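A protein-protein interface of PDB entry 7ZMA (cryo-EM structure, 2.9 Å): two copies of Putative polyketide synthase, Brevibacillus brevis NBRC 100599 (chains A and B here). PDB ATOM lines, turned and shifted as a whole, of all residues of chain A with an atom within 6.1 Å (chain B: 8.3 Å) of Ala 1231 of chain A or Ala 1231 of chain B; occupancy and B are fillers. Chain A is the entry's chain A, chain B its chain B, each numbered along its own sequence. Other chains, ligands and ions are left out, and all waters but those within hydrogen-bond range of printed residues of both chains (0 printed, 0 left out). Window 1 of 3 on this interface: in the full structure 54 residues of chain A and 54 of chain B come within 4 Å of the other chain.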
ATOM      1  N   VAL A1183      -6.584 -30.750   3.698  1.00  0.00           N
ATOM      2  CA  VAL A1183      -6.974 -29.353   3.850  1.00  0.00           C
ATOM      3  C   VAL A1183      -7.728 -29.208   5.164  1.00  0.00           C
ATOM      4  O   VAL A1183      -8.716 -29.914   5.397  1.00  0.00           O
ATOM      5  CB  VAL A1183      -7.838 -28.867   2.674  1.00  0.00           C
ATOM      6  CG1 VAL A1183      -8.342 -27.458   2.925  1.00  0.00           C
ATOM      7  CG2 VAL A1183      -7.049 -28.924   1.384  1.00  0.00           C
ATOM      8  N   TYR A1184      -7.268 -28.294   6.018  1.00  0.00           N
ATOM      9  CA  TYR A1184      -7.908 -28.013   7.295  1.00  0.00           C
ATOM     10  C   TYR A1184      -8.015 -26.507   7.477  1.00  0.00           C
ATOM     11  O   TYR A1184      -7.015 -25.789   7.366  1.00  0.00           O
ATOM     12  CB  TYR A1184      -7.123 -28.639   8.451  1.00  0.00           C
ATOM     13  CG  TYR A1184      -6.941 -30.135   8.324  1.00  0.00           C
ATOM     14  CD1 TYR A1184      -5.902 -30.666   7.573  1.00  0.00           C
ATOM     15  CD2 TYR A1184      -7.805 -31.017   8.955  1.00  0.00           C
ATOM     16  CE1 TYR A1184      -5.731 -32.028   7.453  1.00  0.00           C
ATOM     17  CE2 TYR A1184      -7.641 -32.382   8.842  1.00  0.00           C
ATOM     18  CZ  TYR A1184      -6.602 -32.882   8.089  1.00  0.00           C
ATOM     19  OH  TYR A1184      -6.432 -34.241   7.972  1.00  0.00           O
ATOM     20  N   VAL A1185      -9.226 -26.033   7.763  1.00  0.00           N
ATOM     21  CA  VAL A1185      -9.517 -24.608   7.850  1.00  0.00           C
ATOM     22  C   VAL A1185     -10.266 -24.330   9.145  1.00  0.00           C
ATOM     23  O   VAL A1185     -11.172 -25.080   9.525  1.00  0.00           O
ATOM     24  CB  VAL A1185     -10.329 -24.119   6.632  1.00  0.00           C
ATOM     25  CG1 VAL A1185     -11.678 -24.811   6.570  1.00  0.00           C
ATOM     26  CG2 VAL A1185     -10.497 -22.608   6.670  1.00  0.00           C
ATOM     27  N   GLY A1186      -9.881 -23.250   9.819  1.00  0.00           N
ATOM     28  CA  GLY A1186     -10.542 -22.811  11.029  1.00  0.00           C
ATOM     29  C   GLY A1186     -11.419 -21.595  10.813  1.00  0.00           C
ATOM     30  O   GLY A1186     -10.937 -20.510  10.466  1.00  0.00           O
ATOM     31  N   VAL A1187     -12.719 -21.779  11.018  1.00  0.00           N
ATOM     32  CA  VAL A1187     -13.712 -20.721  10.877  1.00  0.00           C
ATOM     33  C   VAL A1187     -14.748 -20.886  11.979  1.00  0.00           C
ATOM     34  O   VAL A1187     -15.151 -22.011  12.293  1.00  0.00           O
ATOM     35  CB  VAL A1187     -14.374 -20.745   9.486  1.00  0.00           C
ATOM     36  CG1 VAL A1187     -15.161 -22.018   9.293  1.00  0.00           C
ATOM     37  CG2 VAL A1187     -15.284 -19.549   9.316  1.00  0.00           C
ATOM     38  N   PRO A1212     -19.770 -24.167   6.359  1.00  0.00           N
ATOM     39  CA  PRO A1212     -18.394 -23.673   6.202  1.00  0.00           C
ATOM     40  C   PRO A1212     -17.400 -24.727   5.739  1.00  0.00           C
ATOM     41  O   PRO A1212     -16.210 -24.431   5.597  1.00  0.00           O
ATOM     42  CB  PRO A1212     -18.048 -23.170   7.609  1.00  0.00           C
ATOM     43  CG  PRO A1212     -18.939 -23.928   8.517  1.00  0.00           C
ATOM     44  CD  PRO A1212     -20.217 -24.112   7.760  1.00  0.00           C
ATOM     45  N   ALA A1213     -17.862 -25.955   5.501  1.00  0.00           N
ATOM     46  CA  ALA A1213     -17.048 -26.954   4.827  1.00  0.00           C
ATOM     47  C   ALA A1213     -16.726 -26.573   3.393  1.00  0.00           C
ATOM     48  O   ALA A1213     -15.689 -26.997   2.872  1.00  0.00           O
ATOM     49  CB  ALA A1213     -17.758 -28.310   4.831  1.00  0.00           C
ATOM     50  N   ILE A1215     -15.562 -23.924   2.337  1.00  0.00           N
ATOM     51  CA  ILE A1215     -14.329 -23.144   2.288  1.00  0.00           C
ATOM     52  C   ILE A1215     -13.142 -24.037   1.952  1.00  0.00           C
ATOM     53  O   ILE A1215     -12.189 -23.603   1.293  1.00  0.00           O
ATOM     54  CB  ILE A1215     -14.124 -22.403   3.622  1.00  0.00           C
ATOM     55  CG1 ILE A1215     -15.235 -21.370   3.826  1.00  0.00           C
ATOM     56  CG2 ILE A1215     -12.765 -21.732   3.659  1.00  0.00           C
ATOM     57  CD1 ILE A1215     -15.398 -20.922   5.251  1.00  0.00           C
ATOM     58  N   ALA A1216     -13.178 -25.292   2.394  1.00  0.00           N
ATOM     59  CA  ALA A1216     -12.122 -26.252   2.099  1.00  0.00           C
ATOM     60  C   ALA A1216     -12.463 -27.180   0.945  1.00  0.00           C
ATOM     61  O   ALA A1216     -11.563 -27.589   0.200  1.00  0.00           O
ATOM     62  CB  ALA A1216     -11.819 -27.096   3.340  1.00  0.00           C
ATOM     63  N   SER A1229     -10.757 -33.188   3.843  1.00  0.00           N
ATOM     64  CA  SER A1229     -11.061 -31.763   3.767  1.00  0.00           C
ATOM     65  C   SER A1229     -12.162 -31.470   4.775  1.00  0.00           C
ATOM     66  O   SER A1229     -13.332 -31.771   4.521  1.00  0.00           O
ATOM     67  CB  SER A1229     -11.491 -31.366   2.355  1.00  0.00           C
ATOM     68  OG  SER A1229     -12.670 -32.048   1.972  1.00  0.00           O
ATOM     69  N   MET A1230     -11.791 -30.885   5.911  1.00  0.00           N
ATOM     70  CA  MET A1230     -12.727 -30.634   6.995  1.00  0.00           C
ATOM     71  C   MET A1230     -12.502 -29.236   7.546  1.00  0.00           C
ATOM     72  O   MET A1230     -11.400 -28.689   7.465  1.00  0.00           O
ATOM     73  CB  MET A1230     -12.575 -31.671   8.117  1.00  0.00           C
ATOM     74  CG  MET A1230     -11.253 -31.596   8.858  1.00  0.00           C
ATOM     75  SD  MET A1230     -11.072 -32.885  10.102  1.00  0.00           S
ATOM     76  CE  MET A1230     -10.755 -34.303   9.058  1.00  0.00           C
ATOM     77  N   ALA A1231     -13.562 -28.664   8.111  1.00  0.00           N
ATOM     78  CA  ALA A1231     -13.520 -27.349   8.747  1.00  0.00           C
ATOM     79  C   ALA A1231     -13.796 -27.537  10.235  1.00  0.00           C
ATOM     80  O   ALA A1231     -14.945 -27.739  10.640  1.00  0.00           O
ATOM     81  CB  ALA A1231     -14.527 -26.399   8.111  1.00  0.00           C
ATOM     82  N   VAL A1232     -12.744 -27.470  11.047  1.00  0.00           N
ATOM     83  CA  VAL A1232     -12.874 -27.584  12.495  1.00  0.00           C
ATOM     84  C   VAL A1232     -13.502 -26.307  13.031  1.00  0.00           C
ATOM     85  O   VAL A1232     -13.581 -25.297  12.323  1.00  0.00           O
ATOM     86  CB  VAL A1232     -11.512 -27.847  13.161  1.00  0.00           C
ATOM     87  CG1 VAL A1232     -10.869 -29.092  12.584  1.00  0.00           C
ATOM     88  CG2 VAL A1232     -10.596 -26.649  12.993  1.00  0.00           C
ATOM     89  N   ASP A1233     -13.952 -26.339  14.285  1.00  0.00           N
ATOM     90  CA  ASP A1233     -14.548 -25.157  14.905  1.00  0.00           C
ATOM     91  C   ASP A1233     -14.338 -25.253  16.413  1.00  0.00           C
ATOM     92  O   ASP A1233     -15.065 -25.975  17.101  1.00  0.00           O
ATOM     93  CB  ASP A1233     -16.024 -25.039  14.556  1.00  0.00           C
ATOM     94  CG  ASP A1233     -16.581 -23.659  14.844  1.00  0.00           C
ATOM     95  OD1 ASP A1233     -16.254 -23.093  15.908  1.00  0.00           O
ATOM     96  OD2 ASP A1233     -17.345 -23.138  14.006  1.00  0.00           O
ATOM     97  N   THR A1234     -13.340 -24.529  16.910  1.00  0.00           N
ATOM     98  CA  THR A1234     -13.168 -24.282  18.332  1.00  0.00           C
ATOM     99  C   THR A1234     -13.002 -22.784  18.529  1.00  0.00           C
ATOM    100  O   THR A1234     -12.308 -22.124  17.750  1.00  0.00           O
ATOM    101  CB  THR A1234     -11.944 -25.031  18.912  1.00  0.00           C
ATOM    102  OG1 THR A1234     -10.658 -24.586  18.445  1.00  0.00           O
ATOM    103  CG2 THR A1234     -12.135 -26.478  19.415  1.00  0.00           C
ATOM    104  N   VAL B1183     -15.018 -35.024  23.111  1.00  0.00           N
ATOM    105  CA  VAL B1183     -16.346 -34.746  22.577  1.00  0.00           C
ATOM    106  C   VAL B1183     -16.195 -34.304  21.128  1.00  0.00           C
ATOM    107  O   VAL B1183     -15.455 -33.357  20.839  1.00  0.00           O
ATOM    108  CB  VAL B1183     -17.082 -33.673  23.395  1.00  0.00           C
ATOM    109  CG1 VAL B1183     -18.400 -33.305  22.740  1.00  0.00           C
ATOM    110  CG2 VAL B1183     -17.312 -34.158  24.810  1.00  0.00           C
ATOM    111  N   TYR B1184     -16.897 -34.984  20.222  1.00  0.00           N
ATOM    112  CA  TYR B1184     -16.886 -34.652  18.804  1.00  0.00           C
ATOM    113  C   TYR B1184     -18.314 -34.661  18.280  1.00  0.00           C
ATOM    114  O   TYR B1184     -19.039 -35.648  18.453  1.00  0.00           O
ATOM    115  CB  TYR B1184     -16.020 -35.636  18.015  1.00  0.00           C
ATOM    116  CG  TYR B1184     -14.590 -35.713  18.501  1.00  0.00           C
ATOM    117  CD1 TYR B1184     -14.239 -36.536  19.561  1.00  0.00           C
ATOM    118  CD2 TYR B1184     -13.589 -34.963  17.899  1.00  0.00           C
ATOM    119  CE1 TYR B1184     -12.937 -36.609  20.009  1.00  0.00           C
ATOM    120  CE2 TYR B1184     -12.283 -35.032  18.340  1.00  0.00           C
ATOM    121  CZ  TYR B1184     -11.964 -35.857  19.395  1.00  0.00           C
ATOM    122  OH  TYR B1184     -10.665 -35.929  19.839  1.00  0.00           O
ATOM    123  N   VAL B1185     -18.713 -33.567  17.635  1.00  0.00           N
ATOM    124  CA  VAL B1185     -20.083 -33.373  17.179  1.00  0.00           C
ATOM    125  C   VAL B1185     -20.067 -32.938  15.721  1.00  0.00           C
ATOM    126  O   VAL B1185     -19.251 -32.101  15.320  1.00  0.00           O
ATOM    127  CB  VAL B1185     -20.831 -32.341  18.050  1.00  0.00           C
ATOM    128  CG1 VAL B1185     -20.170 -30.978  17.958  1.00  0.00           C
ATOM    129  CG2 VAL B1185     -22.296 -32.260  17.649  1.00  0.00           C
ATOM    130  N   GLY B1186     -20.970 -33.514  14.933  1.00  0.00           N
ATOM    131  CA  GLY B1186     -21.129 -33.154  13.540  1.00  0.00           C
ATOM    132  C   GLY B1186     -22.363 -32.313  13.285  1.00  0.00           C
ATOM    133  O   GLY B1186     -23.498 -32.761  13.488  1.00  0.00           O
ATOM    134  N   VAL B1187     -22.137 -31.080  12.841  1.00  0.00           N
ATOM    135  CA  VAL B1187     -23.200 -30.135  12.523  1.00  0.00           C
ATOM    136  C   VAL B1187     -22.794 -29.357  11.282  1.00  0.00           C
ATOM    137  O   VAL B1187     -21.628 -28.976  11.137  1.00  0.00           O
ATOM    138  CB  VAL B1187     -23.486 -29.186  13.704  1.00  0.00           C
ATOM    139  CG1 VAL B1187     -22.287 -28.313  13.986  1.00  0.00           C
ATOM    140  CG2 VAL B1187     -24.689 -28.321  13.402  1.00  0.00           C
ATOM    141  N   MET B1188     -23.755 -29.120  10.386  1.00  0.00           N
ATOM    142  CA  MET B1188     -23.467 -28.399   9.151  1.00  0.00           C
ATOM    143  C   MET B1188     -23.659 -26.897   9.324  1.00  0.00           C
ATOM    144  O   MET B1188     -22.721 -26.114   9.144  1.00  0.00           O
ATOM    145  CB  MET B1188     -24.362 -28.912   8.021  1.00  0.00           C
ATOM    146  CG  MET B1188     -23.859 -30.160   7.332  1.00  0.00           C
ATOM    147  SD  MET B1188     -25.052 -30.780   6.137  1.00  0.00           S
ATOM    148  CE  MET B1188     -24.761 -29.662   4.773  1.00  0.00           C
ATOM    149  N   GLU B1190     -26.082 -23.484  11.342  1.00  0.00           N
ATOM    150  CA  GLU B1190     -26.974 -22.955  12.363  1.00  0.00           C
ATOM    151  C   GLU B1190     -27.885 -21.926  11.715  1.00  0.00           C
ATOM    152  O   GLU B1190     -27.407 -20.927  11.168  1.00  0.00           O
ATOM    153  CB  GLU B1190     -26.188 -22.329  13.516  1.00  0.00           C
ATOM    154  CG  GLU B1190     -25.144 -23.248  14.121  1.00  0.00           C
ATOM    155  CD  GLU B1190     -24.987 -23.044  15.613  1.00  0.00           C
ATOM    156  OE1 GLU B1190     -24.908 -21.876  16.047  1.00  0.00           O
ATOM    157  OE2 GLU B1190     -24.945 -24.048  16.353  1.00  0.00           O
ATOM    158  N   SER B1211     -21.393 -20.068  16.283  1.00  0.00           N
ATOM    159  CA  SER B1211     -20.205 -20.763  16.755  1.00  0.00           C
ATOM    160  C   SER B1211     -20.585 -22.179  17.171  1.00  0.00           C
ATOM    161  O   SER B1211     -20.657 -22.477  18.369  1.00  0.00           O
ATOM    162  CB  SER B1211     -19.552 -20.019  17.920  1.00  0.00           C
ATOM    163  OG  SER B1211     -18.320 -20.623  18.278  1.00  0.00           O
ATOM    164  N   PRO B1212     -20.846 -23.076  16.213  1.00  0.00           N
ATOM    165  CA  PRO B1212     -21.361 -24.407  16.563  1.00  0.00           C
ATOM    166  C   PRO B1212     -20.437 -25.224  17.453  1.00  0.00           C
ATOM    167  O   PRO B1212     -20.757 -26.368  17.789  1.00  0.00           O
ATOM    168  CB  PRO B1212     -21.538 -25.076  15.193  1.00  0.00           C
ATOM    169  CG  PRO B1212     -20.598 -24.367  14.296  1.00  0.00           C
ATOM    170  CD  PRO B1212     -20.587 -22.948  14.769  1.00  0.00           C
ATOM    171  N   ALA B1213     -19.293 -24.661  17.841  1.00  0.00           N
ATOM    172  CA  ALA B1213     -18.468 -25.258  18.880  1.00  0.00           C
ATOM    173  C   ALA B1213     -19.159 -25.279  20.233  1.00  0.00           C
ATOM    174  O   ALA B1213     -18.861 -26.155  21.051  1.00  0.00           O
ATOM    175  CB  ALA B1213     -17.146 -24.499  19.011  1.00  0.00           C
ATOM    176  N   SER B1214     -20.068 -24.335  20.484  1.00  0.00           N
ATOM    177  CA  SER B1214     -20.811 -24.329  21.738  1.00  0.00           C
ATOM    178  C   SER B1214     -21.501 -25.662  21.983  1.00  0.00           C
ATOM    179  O   SER B1214     -21.578 -26.116  23.129  1.00  0.00           O
ATOM    180  CB  SER B1214     -21.840 -23.200  21.727  1.00  0.00           C
ATOM    181  OG  SER B1214     -21.210 -21.936  21.635  1.00  0.00           O
ATOM    182  N   ILE B1215     -21.976 -26.314  20.922  1.00  0.00           N
ATOM    183  CA  ILE B1215     -22.747 -27.545  21.074  1.00  0.00           C
ATOM    184  C   ILE B1215     -21.952 -28.585  21.852  1.00  0.00           C
ATOM    185  O   ILE B1215     -22.521 -29.392  22.597  1.00  0.00           O
ATOM    186  CB  ILE B1215     -23.174 -28.071  19.692  1.00  0.00           C
ATOM    187  CG1 ILE B1215     -24.135 -27.085  19.027  1.00  0.00           C
ATOM    188  CG2 ILE B1215     -23.820 -29.438  19.814  1.00  0.00           C
ATOM    189  CD1 ILE B1215     -24.255 -27.257  17.538  1.00  0.00           C
ATOM    190  N   ALA B1216     -20.630 -28.584  21.696  1.00  0.00           N
ATOM    191  CA  ALA B1216     -19.759 -29.501  22.420  1.00  0.00           C
ATOM    192  C   ALA B1216     -19.112 -28.872  23.642  1.00  0.00           C
ATOM    193  O   ALA B1216     -18.879 -29.566  24.639  1.00  0.00           O
ATOM    194  CB  ALA B1216     -18.660 -30.024  21.491  1.00  0.00           C
ATOM    195  N   ASN B1217     -18.813 -27.573  23.584  1.00  0.00           N
ATOM    196  CA  ASN B1217     -18.170 -26.913  24.713  1.00  0.00           C
ATOM    197  C   ASN B1217     -19.094 -26.866  25.923  1.00  0.00           C
ATOM    198  O   ASN B1217     -18.645 -27.058  27.056  1.00  0.00           O
ATOM    199  CB  ASN B1217     -17.727 -25.510  24.308  1.00  0.00           C
ATOM    200  CG  ASN B1217     -16.506 -25.525  23.411  1.00  0.00           C
ATOM    201  OD1 ASN B1217     -15.971 -26.585  23.090  1.00  0.00           O
ATOM    202  ND2 ASN B1217     -16.062 -24.347  22.998  1.00  0.00           N
ATOM    203  N   PRO B1228     -10.324 -32.941  24.383  1.00  0.00           N
ATOM    204  CA  PRO B1228     -10.653 -32.120  23.213  1.00  0.00           C
ATOM    205  C   PRO B1228     -12.152 -32.049  22.973  1.00  0.00           C
ATOM    206  O   PRO B1228     -12.877 -33.031  23.142  1.00  0.00           O
ATOM    207  CB  PRO B1228      -9.932 -32.833  22.062  1.00  0.00           C
ATOM    208  CG  PRO B1228      -9.499 -34.158  22.606  1.00  0.00           C
ATOM    209  CD  PRO B1228      -9.327 -33.971  24.067  1.00  0.00           C
ATOM    210  N   SER B1229     -12.609 -30.867  22.569  1.00  0.00           N
ATOM    211  CA  SER B1229     -14.016 -30.624  22.267  1.00  0.00           C
ATOM    212  C   SER B1229     -14.077 -29.785  20.999  1.00  0.00           C
ATOM    213  O   SER B1229     -13.840 -28.574  21.044  1.00  0.00           O
ATOM    214  CB  SER B1229     -14.717 -29.919  23.426  1.00  0.00           C
ATOM    215  OG  SER B1229     -14.136 -28.651  23.675  1.00  0.00           O
ATOM    216  N   MET B1230     -14.394 -30.423  19.875  1.00  0.00           N
ATOM    217  CA  MET B1230     -14.397 -29.758  18.581  1.00  0.00           C
ATOM    218  C   MET B1230     -15.639 -30.168  17.804  1.00  0.00           C
ATOM    219  O   MET B1230     -16.190 -31.252  18.010  1.00  0.00           O
ATOM    220  CB  MET B1230     -13.137 -30.100  17.773  1.00  0.00           C
ATOM    221  CG  MET B1230     -13.046 -31.553  17.348  1.00  0.00           C
ATOM    222  SD  MET B1230     -11.513 -31.936  16.486  1.00  0.00           S
ATOM    223  CE  MET B1230     -10.362 -31.948  17.856  1.00  0.00           C
ATOM    224  N   ALA B1231     -16.071 -29.285  16.908  1.00  0.00           N
ATOM    225  CA  ALA B1231     -17.211 -29.530  16.027  1.00  0.00           C
ATOM    226  C   ALA B1231     -16.698 -29.575  14.593  1.00  0.00           C
ATOM    227  O   ALA B1231     -16.411 -28.533  13.995  1.00  0.00           O
ATOM    228  CB  ALA B1231     -18.279 -28.457  16.201  1.00  0.00           C
ATOM    229  N   VAL B1232     -16.582 -30.780  14.041  1.00  0.00           N
ATOM    230  CA  VAL B1232     -16.150 -30.963  12.661  1.00  0.00           C
ATOM    231  C   VAL B1232     -17.275 -30.531  11.735  1.00  0.00           C
ATOM    232  O   VAL B1232     -18.417 -30.350  12.171  1.00  0.00           O
ATOM    233  CB  VAL B1232     -15.744 -32.422  12.389  1.00  0.00           C
ATOM    234  CG1 VAL B1232     -14.659 -32.861  13.350  1.00  0.00           C
ATOM    235  CG2 VAL B1232     -16.950 -33.338  12.492  1.00  0.00           C
ATOM    236  N   ASP B1233     -16.965 -30.362  10.449  1.00  0.00           N
ATOM    237  CA  ASP B1233     -17.979 -29.976   9.471  1.00  0.00           C
ATOM    238  C   ASP B1233     -17.551 -30.504   8.106  1.00  0.00           C
ATOM    239  O   ASP B1233     -16.694 -29.908   7.445  1.00  0.00           O
ATOM    240  CB  ASP B1233     -18.173 -28.467   9.448  1.00  0.00           C
ATOM    241  CG  ASP B1233     -19.455 -28.056   8.750  1.00  0.00           C
ATOM    242  OD1 ASP B1233     -19.768 -28.634   7.690  1.00  0.00           O
ATOM    243  OD2 ASP B1233     -20.149 -27.154   9.264  1.00  0.00           O
ATOM    244  N   THR B1234     -18.146 -31.621   7.699  1.00  0.00           N
ATOM    245  CA  THR B1234     -18.071 -32.111   6.332  1.00  0.00           C
ATOM    246  C   THR B1234     -19.486 -32.389   5.858  1.00  0.00           C
ATOM    247  O   THR B1234     -20.304 -32.929   6.609  1.00  0.00           O
ATOM    248  CB  THR B1234     -17.212 -33.392   6.216  1.00  0.00           C
ATOM    249  OG1 THR B1234     -17.748 -34.566   6.850  1.00  0.00           O
ATOM    250  CG2 THR B1234     -15.689 -33.243   6.009  1.00  0.00           C
ATOM    251  N   MET B1235     -19.779 -32.010   4.619  1.00  0.00           N
ATOM    252  CA  MET B1235     -21.131 -32.150   4.101  1.00  0.00           C
ATOM    253  C   MET B1235     -21.583 -33.602   4.193  1.00  0.00           C
ATOM    254  O   MET B1235     -20.933 -34.500   3.652  1.00  0.00           O
ATOM    255  CB  MET B1235     -21.192 -31.665   2.653  1.00  0.00           C
ATOM    256  CG  MET B1235     -20.974 -30.173   2.478  1.00  0.00           C
ATOM    257  SD  MET B1235     -21.053 -29.677   0.748  1.00  0.00           S
ATOM    258  CE  MET B1235     -20.671 -27.933   0.869  1.00  0.00           C
ATOM    259  N   SER B1238     -20.340 -35.449   8.564  1.00  0.00           N
ATOM    260  CA  SER B1238     -19.729 -34.886   9.761  1.00  0.00           C
ATOM    261  C   SER B1238     -19.668 -35.905  10.890  1.00  0.00           C
ATOM    262  O   SER B1238     -18.668 -35.975  11.612  1.00  0.00           O
ATOM    263  CB  SER B1238     -20.505 -33.648  10.198  1.00  0.00           C
ATOM    264  OG  SER B1238     -20.596 -32.708   9.144  1.00  0.00           O
ATOM    265  N   THR B1241     -16.891 -38.397  10.170  1.00  0.00           N
ATOM    266  CA  THR B1241     -15.595 -37.758  10.390  1.00  0.00           C
ATOM    267  C   THR B1241     -15.303 -37.602  11.879  1.00  0.00           C
ATOM    268  O   THR B1241     -14.164 -37.792  12.322  1.00  0.00           O
ATOM    269  CB  THR B1241     -15.549 -36.400   9.692  1.00  0.00           C
ATOM    270  OG1 THR B1241     -16.647 -35.592  10.131  1.00  0.00           O
ATOM    271  CG2 THR B1241     -15.615 -36.573   8.186  1.00  0.00           C
ATOM    272  N   GLY B1242     -16.317 -37.238  12.665  1.00  0.00           N
ATOM    273  CA  GLY B1242     -16.125 -37.132  14.100  1.00  0.00           C
ATOM    274  C   GLY B1242     -15.751 -38.458  14.731  1.00  0.00           C
ATOM    275  O   GLY B1242     -14.876 -38.519  15.597  1.00  0.00           O
ATOM    276  N   LEU B1245     -12.094 -39.159  13.887  1.00  0.00           N
ATOM    277  CA  LEU B1245     -11.152 -38.420  14.721  1.00  0.00           C
ATOM    278  C   LEU B1245     -11.141 -38.952  16.148  1.00  0.00           C
ATOM    279  O   LEU B1245     -10.079 -39.055  16.770  1.00  0.00           O
ATOM    280  CB  LEU B1245     -11.496 -36.932  14.709  1.00  0.00           C
ATOM    281  CG  LEU B1245     -11.495 -36.246  13.343  1.00  0.00           C
ATOM    282  CD1 LEU B1245     -12.022 -34.836  13.471  1.00  0.00           C
ATOM    283  CD2 LEU B1245     -10.107 -36.235  12.735  1.00  0.00           C
ATOM    284  N   GLY B1261     -20.896 -37.852  17.890  1.00  0.00           N
ATOM    285  CA  GLY B1261     -22.298 -37.711  17.556  1.00  0.00           C
ATOM    286  C   GLY B1261     -22.527 -36.689  16.468  1.00  0.00           C
ATOM    287  O   GLY B1261     -21.592 -36.143  15.886  1.00  0.00           O
ATOM    288  N   VAL B1263     -25.884 -33.792  14.886  1.00  0.00           N
ATOM    289  CA  VAL B1263     -27.147 -33.109  15.154  1.00  0.00           C
ATOM    290  C   VAL B1263     -27.548 -32.290  13.937  1.00  0.00           C
ATOM    291  O   VAL B1263     -26.705 -31.677  13.277  1.00  0.00           O
ATOM    292  CB  VAL B1263     -27.045 -32.223  16.415  1.00  0.00           C
ATOM    293  CG1 VAL B1263     -25.999 -31.138  16.227  1.00  0.00           C
ATOM    294  CG2 VAL B1263     -28.396 -31.623  16.759  1.00  0.00           C
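The backbone carbonyl oxygen of Ala 1231 of chain A sits at hydrogen-bond distance from the backbone NH of Asp 1233 of chain B, at 3.3 Å.
The backbone NH (N) of Asp 1233 of chain A lies within hydrogen-bond range of the backbone carbonyl oxygen (O) of Ala 1231 of chain B, at 3.3 Å.
Met 1188 of chain B touches Pro 1212 of chain A.
Pro 1212 of chain A touches Asp 1233 of chain B (CD to OD2, 3.4 Å).
O of Asp 1233 of chain B touches CB of Ala 1213 of chain A, at 3.2 Å.
O of Ser 1229 of chain A touches CG2 of Thr 1234 of chain B (3.2 Å).
Ala 1231 of chain A touches Ala 1231 of chain B (O to O, 3.7 Å).
C of Val 1232 of chain A touches O of Ala 1231 of chain B, at 3.8 Å.
Ser 1211 of chain B touches Asp 1233 of chain A (OG to OD1, 3.998 Å).
Pro 1212 of chain B touches Asp 1233 of chain A (CD to OD2, 3.3 Å).
Ala 1213 of chain B touches Asp 1233 of chain A (CB to O, 3.2 Å).
Ser 1229 of chain B touches Thr 1234 of chain A.
Pro 1212 of chain A touches Asp 1233 of chain B, and with the chains exchanged Asp 1233 of chain A touches Pro 1212 of chain B.
Ser 1229 of chain A touches Thr 1234 of chain B, and with the chains exchanged Thr 1234 of chain A touches Ser 1229 of chain B.
Ala 1231 of chain B touches its own counterpart, Ala 1231 of chain A.
Ala 1231 of chain A touches Asp 1233 of chain B, and with the chains exchanged Asp 1233 of chain A touches Ala 1231 of chain B.
Of the 13 pairs that touch across the chains among the printed residues, 11 have their exchanged pair printed and touching as well.
Of the 28 printed residues of chain B, 9 touch a printed residue of chain A.
Printed residues of chain B that touch a printed residue of chain A: Met 1188, Ser 1211, Pro 1212, Ala 1213, Ser 1229, Ala 1231, Val 1232, Asp 1233 and Thr 1234.
Hydrophobic or aromatic side chains of chain B within 4 Å of the printed part of chain A: Pro 1212 and Ala 1213.
Hydrophobic or aromatic side chains of chain A that line the printed part of chain B: Pro 1212 and Ala 1213.
Among the printed residues, no Asp or Glu carboxylate lies within 4 Å of a Lys or Arg side-chain nitrogen of the other chain.
O of Val 1185 of chain A is in hydrogen-bond range of N of Val 1232 of chain A (3.2 Å).
The backbone carbonyl oxygen (O) of Val 1185 of chain B lies within hydrogen-bond range of the backbone NH (N) of Val 1232 of chain B, at 3.2 Å.
The backbone carbonyl oxygen (O) of Ser 1211 of chain B is in hydrogen-bond range of the side-chain hydroxyl (OG) of Ser 1214 of chain B (3.4 Å).
The side-chain hydroxyl of Ser 1229 of chain B lies within hydrogen-bond range of the side-chain amide oxygen of Asn 1217 of chain B (2.8 Å).
The backbone carbonyl oxygen (O) of Thr 1234 of chain B is in hydrogen-bond range of the side-chain hydroxyl (OG) of Ser 1238 of chain B (2.6 Å).
Ala 1231 of chain A touches just these residues of chain B: Ala 1231 (3.7 Å), Val 1232 (3.8 Å) and Asp 1233 (3.3 Å).
Of the printed residues of chain B, Val 1232 of chain A touches Ala 1231 (3.8 Å).
Of the printed residues of chain A, Pro 1212 of chain B touches Asp 1233 (3.3 Å).
Pro 1228 of chain B touches none of the printed residues of chain A.
Printed residues of chain A within 4 Å of Ala 1231 of chain B: Ala 1231 (3.7 Å), Val 1232 (3.8 Å) and Asp 1233 (3.3 Å).
Of the printed residues of chain A, Val 1232 of chain B touches Ala 1231 (3.8 Å).
The nearest residue of chain A that does not touch Ala 1231 of chain B is Thr 1234 of chain A (5.4 Å).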
